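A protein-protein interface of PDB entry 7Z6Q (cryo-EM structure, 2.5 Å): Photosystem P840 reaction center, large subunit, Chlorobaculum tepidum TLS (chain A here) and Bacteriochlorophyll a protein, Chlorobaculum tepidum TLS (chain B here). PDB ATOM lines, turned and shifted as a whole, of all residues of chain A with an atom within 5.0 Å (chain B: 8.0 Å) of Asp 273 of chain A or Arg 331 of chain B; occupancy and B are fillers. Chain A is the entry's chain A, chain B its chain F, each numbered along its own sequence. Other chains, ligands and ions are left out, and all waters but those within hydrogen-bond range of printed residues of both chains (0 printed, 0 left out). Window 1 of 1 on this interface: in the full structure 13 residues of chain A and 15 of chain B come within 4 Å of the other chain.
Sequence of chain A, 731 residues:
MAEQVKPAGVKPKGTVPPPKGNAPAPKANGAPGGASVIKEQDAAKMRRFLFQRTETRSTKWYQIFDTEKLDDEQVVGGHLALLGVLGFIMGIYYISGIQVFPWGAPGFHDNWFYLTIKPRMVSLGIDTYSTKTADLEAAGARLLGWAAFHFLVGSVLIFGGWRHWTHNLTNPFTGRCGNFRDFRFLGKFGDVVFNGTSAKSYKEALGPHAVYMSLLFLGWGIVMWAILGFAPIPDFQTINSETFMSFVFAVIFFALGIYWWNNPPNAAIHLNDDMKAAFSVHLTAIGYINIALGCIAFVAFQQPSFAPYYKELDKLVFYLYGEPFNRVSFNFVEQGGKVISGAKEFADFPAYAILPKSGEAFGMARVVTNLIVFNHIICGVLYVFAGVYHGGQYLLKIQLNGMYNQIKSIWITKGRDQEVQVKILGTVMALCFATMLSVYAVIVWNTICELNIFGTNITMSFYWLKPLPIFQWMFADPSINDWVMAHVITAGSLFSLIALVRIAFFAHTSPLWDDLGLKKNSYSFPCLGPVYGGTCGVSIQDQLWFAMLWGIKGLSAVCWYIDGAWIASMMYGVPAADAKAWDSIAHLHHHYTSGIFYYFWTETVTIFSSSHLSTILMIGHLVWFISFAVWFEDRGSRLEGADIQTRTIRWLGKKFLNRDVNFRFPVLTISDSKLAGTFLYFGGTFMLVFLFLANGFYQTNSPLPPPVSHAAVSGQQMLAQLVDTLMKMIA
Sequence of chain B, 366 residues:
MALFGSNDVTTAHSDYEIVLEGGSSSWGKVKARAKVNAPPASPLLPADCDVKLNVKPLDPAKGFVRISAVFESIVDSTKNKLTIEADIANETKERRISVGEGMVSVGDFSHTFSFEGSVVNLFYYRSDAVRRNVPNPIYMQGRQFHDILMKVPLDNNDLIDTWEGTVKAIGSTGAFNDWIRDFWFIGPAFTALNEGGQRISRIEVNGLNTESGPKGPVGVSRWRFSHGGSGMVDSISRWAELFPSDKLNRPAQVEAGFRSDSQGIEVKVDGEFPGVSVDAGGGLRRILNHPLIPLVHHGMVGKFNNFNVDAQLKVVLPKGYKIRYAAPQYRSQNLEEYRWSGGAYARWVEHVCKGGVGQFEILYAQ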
ATOM      1  N   ASP A  72      20.910   3.067  13.734  1.00  0.00           N
ATOM      2  CA  ASP A  72      19.836   2.063  13.476  1.00  0.00           C
ATOM      3  C   ASP A  72      18.419   2.636  13.630  1.00  0.00           C
ATOM      4  O   ASP A  72      17.495   2.052  13.040  1.00  0.00           O
ATOM      5  CB  ASP A  72      20.040   0.786  14.293  1.00  0.00           C
ATOM      6  CG  ASP A  72      19.009  -0.274  13.964  1.00  0.00           C
ATOM      7  OD1 ASP A  72      17.896  -0.181  14.509  1.00  0.00           O
ATOM      8  OD2 ASP A  72      19.318  -1.168  13.158  1.00  0.00           O
ATOM      9  N   LYS A 200      18.645  -6.403  21.295  1.00  0.00           N
ATOM     10  CA  LYS A 200      19.726  -5.385  21.402  1.00  0.00           C
ATOM     11  C   LYS A 200      20.690  -5.495  20.214  1.00  0.00           C
ATOM     12  O   LYS A 200      21.513  -4.577  20.039  1.00  0.00           O
ATOM     13  CB  LYS A 200      20.507  -5.576  22.706  1.00  0.00           C
ATOM     14  CG  LYS A 200      19.707  -6.106  23.886  1.00  0.00           C
ATOM     15  CD  LYS A 200      18.848  -5.057  24.547  1.00  0.00           C
ATOM     16  CE  LYS A 200      17.926  -5.636  25.599  1.00  0.00           C
ATOM     17  NZ  LYS A 200      16.972  -4.623  26.106  1.00  0.00           N
ATOM     18  N   TYR A 202      21.278  -7.121  15.868  1.00  0.00           N
ATOM     19  CA  TYR A 202      20.591  -7.576  14.632  1.00  0.00           C
ATOM     20  C   TYR A 202      20.300  -9.076  14.707  1.00  0.00           C
ATOM     21  O   TYR A 202      19.188  -9.463  14.334  1.00  0.00           O
ATOM     22  CB  TYR A 202      21.415  -7.279  13.376  1.00  0.00           C
ATOM     23  CG  TYR A 202      21.628  -5.819  13.069  1.00  0.00           C
ATOM     24  CD1 TYR A 202      20.710  -5.096  12.327  1.00  0.00           C
ATOM     25  CD2 TYR A 202      22.762  -5.163  13.512  1.00  0.00           C
ATOM     26  CE1 TYR A 202      20.905  -3.756  12.045  1.00  0.00           C
ATOM     27  CE2 TYR A 202      22.975  -3.823  13.239  1.00  0.00           C
ATOM     28  CZ  TYR A 202      22.044  -3.117  12.501  1.00  0.00           C
ATOM     29  OH  TYR A 202      22.253  -1.796  12.232  1.00  0.00           O
ATOM     30  N   ILE A 269      28.180 -13.471  11.859  1.00  0.00           N
ATOM     31  CA  ILE A 269      28.180 -12.580  13.059  1.00  0.00           C
ATOM     32  C   ILE A 269      28.788 -11.219  12.699  1.00  0.00           C
ATOM     33  O   ILE A 269      28.236 -10.202  13.153  1.00  0.00           O
ATOM     34  CB  ILE A 269      28.901 -13.243  14.252  1.00  0.00           C
ATOM     35  CG1 ILE A 269      28.776 -12.400  15.522  1.00  0.00           C
ATOM     36  CG2 ILE A 269      30.361 -13.509  13.926  1.00  0.00           C
ATOM     37  CD1 ILE A 269      29.185 -13.127  16.781  1.00  0.00           C
ATOM     38  N   HIS A 270      29.850 -11.208  11.888  1.00  0.00           N
ATOM     39  CA  HIS A 270      30.538  -9.951  11.485  1.00  0.00           C
ATOM     40  C   HIS A 270      29.533  -8.904  10.985  1.00  0.00           C
ATOM     41  O   HIS A 270      29.849  -7.701  11.074  1.00  0.00           O
ATOM     42  CB  HIS A 270      31.621 -10.248  10.438  1.00  0.00           C
ATOM     43  CG  HIS A 270      31.089 -10.832   9.173  1.00  0.00           C
ATOM     44  ND1 HIS A 270      30.950 -12.194   8.990  1.00  0.00           N
ATOM     45  CD2 HIS A 270      30.663 -10.251   8.031  1.00  0.00           C
ATOM     46  CE1 HIS A 270      30.461 -12.428   7.789  1.00  0.00           C
ATOM     47  NE2 HIS A 270      30.276 -11.250   7.180  1.00  0.00           N
ATOM     48  N   LEU A 271      28.373  -9.342  10.481  1.00  0.00           N
ATOM     49  CA  LEU A 271      27.345  -8.409   9.947  1.00  0.00           C
ATOM     50  C   LEU A 271      26.754  -7.567  11.086  1.00  0.00           C
ATOM     51  O   LEU A 271      26.544  -6.361  10.868  1.00  0.00           O
ATOM     52  CB  LEU A 271      26.248  -9.233   9.268  1.00  0.00           C
ATOM     53  CG  LEU A 271      26.695 -10.075   8.076  1.00  0.00           C
ATOM     54  CD1 LEU A 271      25.493 -10.654   7.352  1.00  0.00           C
ATOM     55  CD2 LEU A 271      27.537  -9.252   7.120  1.00  0.00           C
ATOM     56  N   ASN A 272      26.511  -8.171  12.252  1.00  0.00           N
ATOM     57  CA  ASN A 272      25.933  -7.438  13.411  1.00  0.00           C
ATOM     58  C   ASN A 272      26.764  -6.199  13.763  1.00  0.00           C
ATOM     59  O   ASN A 272      26.210  -5.304  14.427  1.00  0.00           O
ATOM     60  CB  ASN A 272      25.860  -8.312  14.664  1.00  0.00           C
ATOM     61  CG  ASN A 272      25.254  -9.672  14.409  1.00  0.00           C
ATOM     62  OD1 ASN A 272      24.233  -9.778  13.740  1.00  0.00           O
ATOM     63  ND2 ASN A 272      25.875 -10.714  14.936  1.00  0.00           N
ATOM     64  N   ASP A 273      28.041  -6.158  13.365  1.00  0.00           N
ATOM     65  CA  ASP A 273      28.908  -5.043  13.730  1.00  0.00           C
ATOM     66  C   ASP A 273      28.696  -3.832  12.831  1.00  0.00           C
ATOM     67  O   ASP A 273      28.742  -2.695  13.311  1.00  0.00           O
ATOM     68  CB  ASP A 273      30.375  -5.484  13.681  1.00  0.00           C
ATOM     69  CG  ASP A 273      30.647  -6.736  14.508  1.00  0.00           C
ATOM     70  OD1 ASP A 273      29.763  -7.166  15.276  1.00  0.00           O
ATOM     71  OD2 ASP A 273      31.740  -7.319  14.353  1.00  0.00           O
ATOM     72  N   ASP A 274      28.468  -4.042  11.536  1.00  0.00           N
ATOM     73  CA  ASP A 274      28.334  -2.936  10.601  1.00  0.00           C
ATOM     74  C   ASP A 274      27.030  -3.066   9.830  1.00  0.00           C
ATOM     75  O   ASP A 274      26.605  -4.174   9.484  1.00  0.00           O
ATOM     76  CB  ASP A 274      29.516  -2.872   9.628  1.00  0.00           C
ATOM     77  CG  ASP A 274      29.504  -1.607   8.787  1.00  0.00           C
ATOM     78  OD1 ASP A 274      28.806  -0.653   9.180  1.00  0.00           O
ATOM     79  OD2 ASP A 274      30.191  -1.558   7.744  1.00  0.00           O
ATOM     80  N   MET A 275      26.381  -1.919   9.619  1.00  0.00           N
ATOM     81  CA  MET A 275      25.066  -1.815   8.934  1.00  0.00           C
ATOM     82  C   MET A 275      25.181  -2.214   7.457  1.00  0.00           C
ATOM     83  O   MET A 275      24.374  -3.057   7.018  1.00  0.00           O
ATOM     84  CB  MET A 275      24.553  -0.374   9.030  1.00  0.00           C
ATOM     85  CG  MET A 275      23.098  -0.211   8.652  1.00  0.00           C
ATOM     86  SD  MET A 275      22.533   1.500   8.823  1.00  0.00           S
ATOM     87  CE  MET A 275      22.646   1.714  10.596  1.00  0.00           C
ATOM     88  N   ALA B 311      24.999  -1.466  26.136  1.00  0.00           N
ATOM     89  CA  ALA B 311      26.011  -0.411  26.379  1.00  0.00           C
ATOM     90  C   ALA B 311      26.260   0.415  25.110  1.00  0.00           C
ATOM     91  O   ALA B 311      26.396  -0.182  24.034  1.00  0.00           O
ATOM     92  CB  ALA B 311      27.295  -1.023  26.883  1.00  0.00           C
ATOM     93  N   GLN B 312      26.337   1.741  25.260  1.00  0.00           N
ATOM     94  CA  GLN B 312      26.601   2.684  24.137  1.00  0.00           C
ATOM     95  C   GLN B 312      27.809   3.558  24.497  1.00  0.00           C
ATOM     96  O   GLN B 312      27.840   4.059  25.629  1.00  0.00           O
ATOM     97  CB  GLN B 312      25.379   3.585  23.951  1.00  0.00           C
ATOM     98  CG  GLN B 312      25.573   4.671  22.902  1.00  0.00           C
ATOM     99  CD  GLN B 312      24.988   4.292  21.565  1.00  0.00           C
ATOM    100  OE1 GLN B 312      23.894   3.737  21.477  1.00  0.00           O
ATOM    101  NE2 GLN B 312      25.719   4.597  20.505  1.00  0.00           N
ATOM    102  N   LEU B 313      28.825   3.567  23.643  1.00  0.00           N
ATOM    103  CA  LEU B 313      30.044   4.315  23.904  1.00  0.00           C
ATOM    104  C   LEU B 313      30.219   5.377  22.847  1.00  0.00           C
ATOM    105  O   LEU B 313      30.645   5.096  21.726  1.00  0.00           O
ATOM    106  CB  LEU B 313      31.253   3.380  23.918  1.00  0.00           C
ATOM    107  CG  LEU B 313      32.627   4.047  23.829  1.00  0.00           C
ATOM    108  CD1 LEU B 313      32.901   4.880  25.071  1.00  0.00           C
ATOM    109  CD2 LEU B 313      33.717   3.005  23.628  1.00  0.00           C
ATOM    110  N   PRO B 328      37.196  -3.449  18.875  1.00  0.00           N
ATOM    111  CA  PRO B 328      36.076  -3.589  17.927  1.00  0.00           C
ATOM    112  C   PRO B 328      35.606  -2.313  17.214  1.00  0.00           C
ATOM    113  O   PRO B 328      35.537  -1.285  17.838  1.00  0.00           O
ATOM    114  CB  PRO B 328      34.900  -4.040  18.808  1.00  0.00           C
ATOM    115  CG  PRO B 328      35.543  -4.592  20.054  1.00  0.00           C
ATOM    116  CD  PRO B 328      36.770  -3.733  20.244  1.00  0.00           C
ATOM    117  N   GLN B 329      35.260  -2.451  15.931  1.00  0.00           N
ATOM    118  CA  GLN B 329      34.991  -1.323  14.996  1.00  0.00           C
ATOM    119  C   GLN B 329      33.728  -0.572  15.437  1.00  0.00           C
ATOM    120  O   GLN B 329      32.806  -1.233  15.952  1.00  0.00           O
ATOM    121  CB  GLN B 329      34.861  -1.882  13.580  1.00  0.00           C
ATOM    122  CG  GLN B 329      34.913  -0.824  12.492  1.00  0.00           C
ATOM    123  CD  GLN B 329      36.113   0.070  12.645  1.00  0.00           C
ATOM    124  OE1 GLN B 329      36.022   1.183  13.153  1.00  0.00           O
ATOM    125  NE2 GLN B 329      37.258  -0.418  12.210  1.00  0.00           N
ATOM    126  N   TYR B 330      33.693   0.751  15.244  1.00  0.00           N
ATOM    127  CA  TYR B 330      32.516   1.552  15.677  1.00  0.00           C
ATOM    128  C   TYR B 330      31.291   1.184  14.838  1.00  0.00           C
ATOM    129  O   TYR B 330      31.407   1.143  13.601  1.00  0.00           O
ATOM    130  CB  TYR B 330      32.802   3.054  15.597  1.00  0.00           C
ATOM    131  CG  TYR B 330      33.502   3.533  14.352  1.00  0.00           C
ATOM    132  CD1 TYR B 330      32.834   3.628  13.145  1.00  0.00           C
ATOM    133  CD2 TYR B 330      34.827   3.924  14.390  1.00  0.00           C
ATOM    134  CE1 TYR B 330      33.471   4.086  12.001  1.00  0.00           C
ATOM    135  CE2 TYR B 330      35.483   4.369  13.254  1.00  0.00           C
ATOM    136  CZ  TYR B 330      34.801   4.460  12.056  1.00  0.00           C
ATOM    137  OH  TYR B 330      35.440   4.912  10.940  1.00  0.00           O
ATOM    138  N   ARG B 331      30.161   0.925  15.503  1.00  0.00           N
ATOM    139  CA  ARG B 331      28.901   0.546  14.808  1.00  0.00           C
ATOM    140  C   ARG B 331      28.529   1.644  13.805  1.00  0.00           C
ATOM    141  O   ARG B 331      28.202   1.301  12.650  1.00  0.00           O
ATOM    142  CB  ARG B 331      27.775   0.328  15.824  1.00  0.00           C
ATOM    143  CG  ARG B 331      26.476  -0.179  15.213  1.00  0.00           C
ATOM    144  CD  ARG B 331      25.666  -1.012  16.189  1.00  0.00           C
ATOM    145  NE  ARG B 331      24.277  -1.154  15.776  1.00  0.00           N
ATOM    146  CZ  ARG B 331      23.329  -1.727  16.509  1.00  0.00           C
ATOM    147  NH1 ARG B 331      23.618  -2.215  17.702  1.00  0.00           N
ATOM    148  NH2 ARG B 331      22.093  -1.809  16.045  1.00  0.00           N
ATOM    149  N   SER B 332      28.580   2.908  14.236  1.00  0.00           N
ATOM    150  CA  SER B 332      28.152   4.041  13.380  1.00  0.00           C
ATOM    151  C   SER B 332      29.175   5.173  13.488  1.00  0.00           C
ATOM    152  O   SER B 332      29.887   5.227  14.500  1.00  0.00           O
ATOM    153  CB  SER B 332      26.766   4.503  13.744  1.00  0.00           C
ATOM    154  OG  SER B 332      26.794   5.353  14.876  1.00  0.00           O
ATOM    155  N   GLN B 333      29.252   6.026  12.469  1.00  0.00           N
ATOM    156  CA  GLN B 333      29.998   7.303  12.587  1.00  0.00           C
ATOM    157  C   GLN B 333      29.028   8.441  12.279  1.00  0.00           C
ATOM    158  O   GLN B 333      28.179   8.261  11.390  1.00  0.00           O
ATOM    159  CB  GLN B 333      31.182   7.342  11.625  1.00  0.00           C
ATOM    160  CG  GLN B 333      31.983   8.627  11.745  1.00  0.00           C
ATOM    161  CD  GLN B 333      32.644   9.040  10.456  1.00  0.00           C
ATOM    162  OE1 GLN B 333      32.899   8.222   9.579  1.00  0.00           O
ATOM    163  NE2 GLN B 333      32.938  10.323  10.339  1.00  0.00           N
ATOM    164  N   ASN B 334      29.135   9.552  12.998  1.00  0.00           N
ATOM    165  CA  ASN B 334      28.279  10.708  12.778  1.00  0.00           C
ATOM    166  C   ASN B 334      29.129  11.963  12.887  1.00  0.00           C
ATOM    167  O   ASN B 334      29.306  12.499  13.984  1.00  0.00           O
ATOM    168  CB  ASN B 334      27.143  10.744  13.799  1.00  0.00           C
ATOM    169  CG  ASN B 334      26.443  12.088  13.844  1.00  0.00           C
ATOM    170  OD1 ASN B 334      26.580  12.903  12.932  1.00  0.00           O
ATOM    171  ND2 ASN B 334      25.685  12.326  14.909  1.00  0.00           N
ATOM    172  N   TYR B 338      32.047   9.370  16.868  1.00  0.00           N
ATOM    173  CA  TYR B 338      31.982   7.948  16.448  1.00  0.00           C
ATOM    174  C   TYR B 338      31.245   7.200  17.558  1.00  0.00           C
ATOM    175  O   TYR B 338      31.428   7.588  18.713  1.00  0.00           O
ATOM    176  CB  TYR B 338      33.391   7.395  16.230  1.00  0.00           C
ATOM    177  CG  TYR B 338      34.194   8.089  15.158  1.00  0.00           C
ATOM    178  CD1 TYR B 338      34.679   9.374  15.340  1.00  0.00           C
ATOM    179  CD2 TYR B 338      34.496   7.454  13.970  1.00  0.00           C
ATOM    180  CE1 TYR B 338      35.424  10.013  14.363  1.00  0.00           C
ATOM    181  CE2 TYR B 338      35.241   8.076  12.985  1.00  0.00           C
ATOM    182  CZ  TYR B 338      35.708   9.360  13.180  1.00  0.00           C
ATOM    183  OH  TYR B 338      36.441   9.976  12.208  1.00  0.00           O
ATOM    184  N   ARG B 339      30.442   6.191  17.212  1.00  0.00           N
ATOM    185  CA  ARG B 339      29.583   5.503  18.213  1.00  0.00           C
ATOM    186  C   ARG B 339      29.966   4.021  18.280  1.00  0.00           C
ATOM    187  O   ARG B 339      30.254   3.437  17.216  1.00  0.00           O
ATOM    188  CB  ARG B 339      28.104   5.668  17.849  1.00  0.00           C
ATOM    189  CG  ARG B 339      27.640   7.115  17.773  1.00  0.00           C
ATOM    190  CD  ARG B 339      26.227   7.295  18.296  1.00  0.00           C
ATOM    191  NE  ARG B 339      25.985   8.644  18.787  1.00  0.00           N
ATOM    192  CZ  ARG B 339      25.122   8.952  19.748  1.00  0.00           C
ATOM    193  NH1 ARG B 339      24.973  10.210  20.126  1.00  0.00           N
ATOM    194  NH2 ARG B 339      24.411   8.001  20.329  1.00  0.00           N
ATOM    195  N   TRP B 340      29.964   3.442  19.486  1.00  0.00           N
ATOM    196  CA  TRP B 340      30.100   1.971  19.631  1.00  0.00           C
ATOM    197  C   TRP B 340      28.853   1.434  20.327  1.00  0.00           C
ATOM    198  O   TRP B 340      28.522   1.930  21.407  1.00  0.00           O
ATOM    199  CB  TRP B 340      31.363   1.623  20.426  1.00  0.00           C
ATOM    200  CG  TRP B 340      32.632   1.732  19.640  1.00  0.00           C
ATOM    201  CD1 TRP B 340      33.348   0.706  19.106  1.00  0.00           C
ATOM    202  CD2 TRP B 340      33.340   2.937  19.304  1.00  0.00           C
ATOM    203  NE1 TRP B 340      34.450   1.189  18.457  1.00  0.00           N
ATOM    204  CE2 TRP B 340      34.473   2.552  18.562  1.00  0.00           C
ATOM    205  CE3 TRP B 340      33.135   4.296  19.557  1.00  0.00           C
ATOM    206  CZ2 TRP B 340      35.387   3.478  18.069  1.00  0.00           C
ATOM    207  CZ3 TRP B 340      34.041   5.211  19.071  1.00  0.00           C
ATOM    208  CH2 TRP B 340      35.152   4.806  18.336  1.00  0.00           C
ATOM    209  N   SER B 341      28.201   0.449  19.724  1.00  0.00           N
ATOM    210  CA  SER B 341      27.081  -0.255  20.388  1.00  0.00           C
ATOM    211  C   SER B 341      26.917  -1.605  19.700  1.00  0.00           C
ATOM    212  O   SER B 341      27.164  -1.673  18.489  1.00  0.00           O
ATOM    213  CB  SER B 341      25.817   0.559  20.325  1.00  0.00           C
ATOM    214  OG  SER B 341      25.387   0.730  18.984  1.00  0.00           O
ATOM    215  N   GLY B 342      26.617  -2.655  20.461  1.00  0.00           N
ATOM    216  CA  GLY B 342      26.122  -3.918  19.878  1.00  0.00           C
ATOM    217  C   GLY B 342      27.219  -4.811  19.308  1.00  0.00           C
ATOM    218  O   GLY B 342      28.396  -4.407  19.278  1.00  0.00           O
ATOM    219  N   GLY B 343      26.841  -5.990  18.816  1.00  0.00           N
ATOM    220  CA  GLY B 343      27.765  -6.800  17.999  1.00  0.00           C
ATOM    221  C   GLY B 343      29.043  -7.125  18.747  1.00  0.00           C
ATOM    222  O   GLY B 343      28.952  -7.772  19.804  1.00  0.00           O
ATOM    223  N   ALA B 344      30.194  -6.705  18.210  1.00  0.00           N
ATOM    224  CA  ALA B 344      31.498  -7.055  18.820  1.00  0.00           C
ATOM    225  C   ALA B 344      31.661  -6.327  20.158  1.00  0.00           C
ATOM    226  O   ALA B 344      32.132  -6.957  21.117  1.00  0.00           O
ATOM    227  CB  ALA B 344      32.615  -6.698  17.873  1.00  0.00           C
ATOM    228  N   TYR B 345      31.279  -5.047  20.198  1.00  0.00           N
ATOM    229  CA  TYR B 345      31.516  -4.175  21.376  1.00  0.00           C
ATOM    230  C   TYR B 345      30.740  -4.702  22.588  1.00  0.00           C
ATOM    231  O   TYR B 345      31.278  -4.637  23.699  1.00  0.00           O
ATOM    232  CB  TYR B 345      31.186  -2.718  21.048  1.00  0.00           C
ATOM    233  CG  TYR B 345      31.180  -1.797  22.241  1.00  0.00           C
ATOM    234  CD1 TYR B 345      32.360  -1.307  22.779  1.00  0.00           C
ATOM    235  CD2 TYR B 345      29.991  -1.413  22.836  1.00  0.00           C
ATOM    236  CE1 TYR B 345      32.358  -0.460  23.873  1.00  0.00           C
ATOM    237  CE2 TYR B 345      29.969  -0.568  23.931  1.00  0.00           C
ATOM    238  CZ  TYR B 345      31.157  -0.092  24.452  1.00  0.00           C
ATOM    239  OH  TYR B 345      31.133   0.739  25.531  1.00  0.00           O
ATOM    240  N   ALA B 346      29.514  -5.185  22.386  1.00  0.00           N
ATOM    241  CA  ALA B 346      28.689  -5.655  23.522  1.00  0.00           C
ATOM    242  C   ALA B 346      29.036  -7.109  23.848  1.00  0.00           C
ATOM    243  O   ALA B 346      28.436  -7.662  24.785  1.00  0.00           O
ATOM    244  CB  ALA B 346      27.227  -5.491  23.207  1.00  0.00           C
ATOM    245  N   ARG B 347      29.951  -7.704  23.077  1.00  0.00           N
ATOM    246  CA  ARG B 347      30.701  -8.921  23.484  1.00  0.00           C
ATOM    247  C   ARG B 347      31.910  -8.485  24.321  1.00  0.00           C
ATOM    248  O   ARG B 347      32.116  -9.079  25.392  1.00  0.00           O
ATOM    249  CB  ARG B 347      31.100  -9.773  22.277  1.00  0.00           C
ATOM    250  CG  ARG B 347      29.920 -10.441  21.585  1.00  0.00           C
ATOM    251  CD  ARG B 347      30.338 -11.516  20.603  1.00  0.00           C
ATOM    252  NE  ARG B 347      31.147 -10.996  19.512  1.00  0.00           N
ATOM    253  CZ  ARG B 347      30.653 -10.478  18.395  1.00  0.00           C
ATOM    254  NH1 ARG B 347      29.355 -10.549  18.151  1.00  0.00           N
ATOM    255  NH2 ARG B 347      31.455  -9.887  17.527  1.00  0.00           N
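OD2 of Asp 72 of chain A sits at hydrogen-bond distance from OH of Tyr 202 of chain A (3.1 Å). The side-chain amide nitrogen (ND2) of Asn 272 of chain A lies within hydrogen-bond range of the backbone carbonyl oxygen (O) of Ile 269 of chain A, at 3.0 Å. The backbone NH of Arg 331 of chain B is in hydrogen-bond range of the backbone carbonyl oxygen of Arg 339 of chain B (3.0 Å). The backbone carbonyl oxygen (O) of Gly 343 of chain B sits at hydrogen-bond distance from the guanidinium group (NH1) of Arg 347 of chain B (3.3 Å).
The side-chain carboxylate (OD1) of Asp 273 of chain A lies within hydrogen-bond range of the backbone NH (N) of Ala 344 of chain B. OD1 of Asp 273 of chain A lies within salt-bridge range of NH2 of Arg 347 of chain B (3.9 Å).
Of the printed residues of chain B, Asp 72 of chain A touches Arg 331 (3.7 Å). Of the printed residues of chain B, Tyr 202 of chain A touches Arg 331 (3.6 Å). Of the printed residues of chain B, Ile 269 of chain A touches Arg 347 (2.9 Å). Of chain B, only Arg 331 (3.6 Å), Gly 343 (3.4 Å), Ala 344 (3.0 Å) and Arg 347 (3.9 Å) come within 4 Å of Asp 273 of chain A. Arg 331 of chain B touches just these residues of chain A: Asp 72 (3.7 Å), Lys 200 (3.9 Å), Tyr 202 (3.6 Å) and Asp 273 (3.6 Å). Gly 342 of chain B touches none of the printed residues of chain A. Of the printed residues of chain A, Gly 343 of chain B touches Asp 273 (3.4 Å). Of the printed residues of chain A, Arg 347 of chain B touches Ile 269 and Asp 273. The nearest residue of chain B that does not touch Asp 273 of chain A is Tyr 330 of chain B (4.7 Å). The nearest residue of chain A that does not touch Arg 331 of chain B is Asp 274 of chain A (4.03 Å). The nearest printed residue of chain A that does not touch Arg 347 of chain B is Asn 272 of chain A (4.7 Å).
Of the 20 printed residues of chain B, 4 touch a printed residue of chain A. Printed residues of chain B that touch a printed residue of chain A: Arg 331, Gly 343, Ala 344 and Arg 347. Hydrophobic or aromatic side chains of chain B that line the printed part of chain A: Ala 344. Of the 10 printed residues of chain A, 5 touch a printed residue of chain B. Printed residues of chain A that touch a printed residue of chain B: Asp 72, Lys 200, Tyr 202, Ile 269 and Asp 273. Hydrophobic or aromatic side chains of chain A that line the printed part of chain B: Tyr 202 and Ile 269. Among the printed residues, 8 pairs touch across the chains. Among the printed residues, Asp or Glu carboxylates within 4 Å of a Lys or Arg side-chain nitrogen of the other chain: Asp 273 of chain A with Arg 347 of chain B (3.9 Å).
Among the printed residues, pairs that only touch across the chains: Ile 269 of chain A with Arg 347 of chain B, Asp 273 of chain A with Gly 343 of chain B, Tyr 202 of chain A with Arg 331 of chain B, Asp 273 of chain A with Arg 331 of chain B, Asp 72 of chain A with Arg 331 of chain B and Lys 200 of chain A with Arg 331 of chain B.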
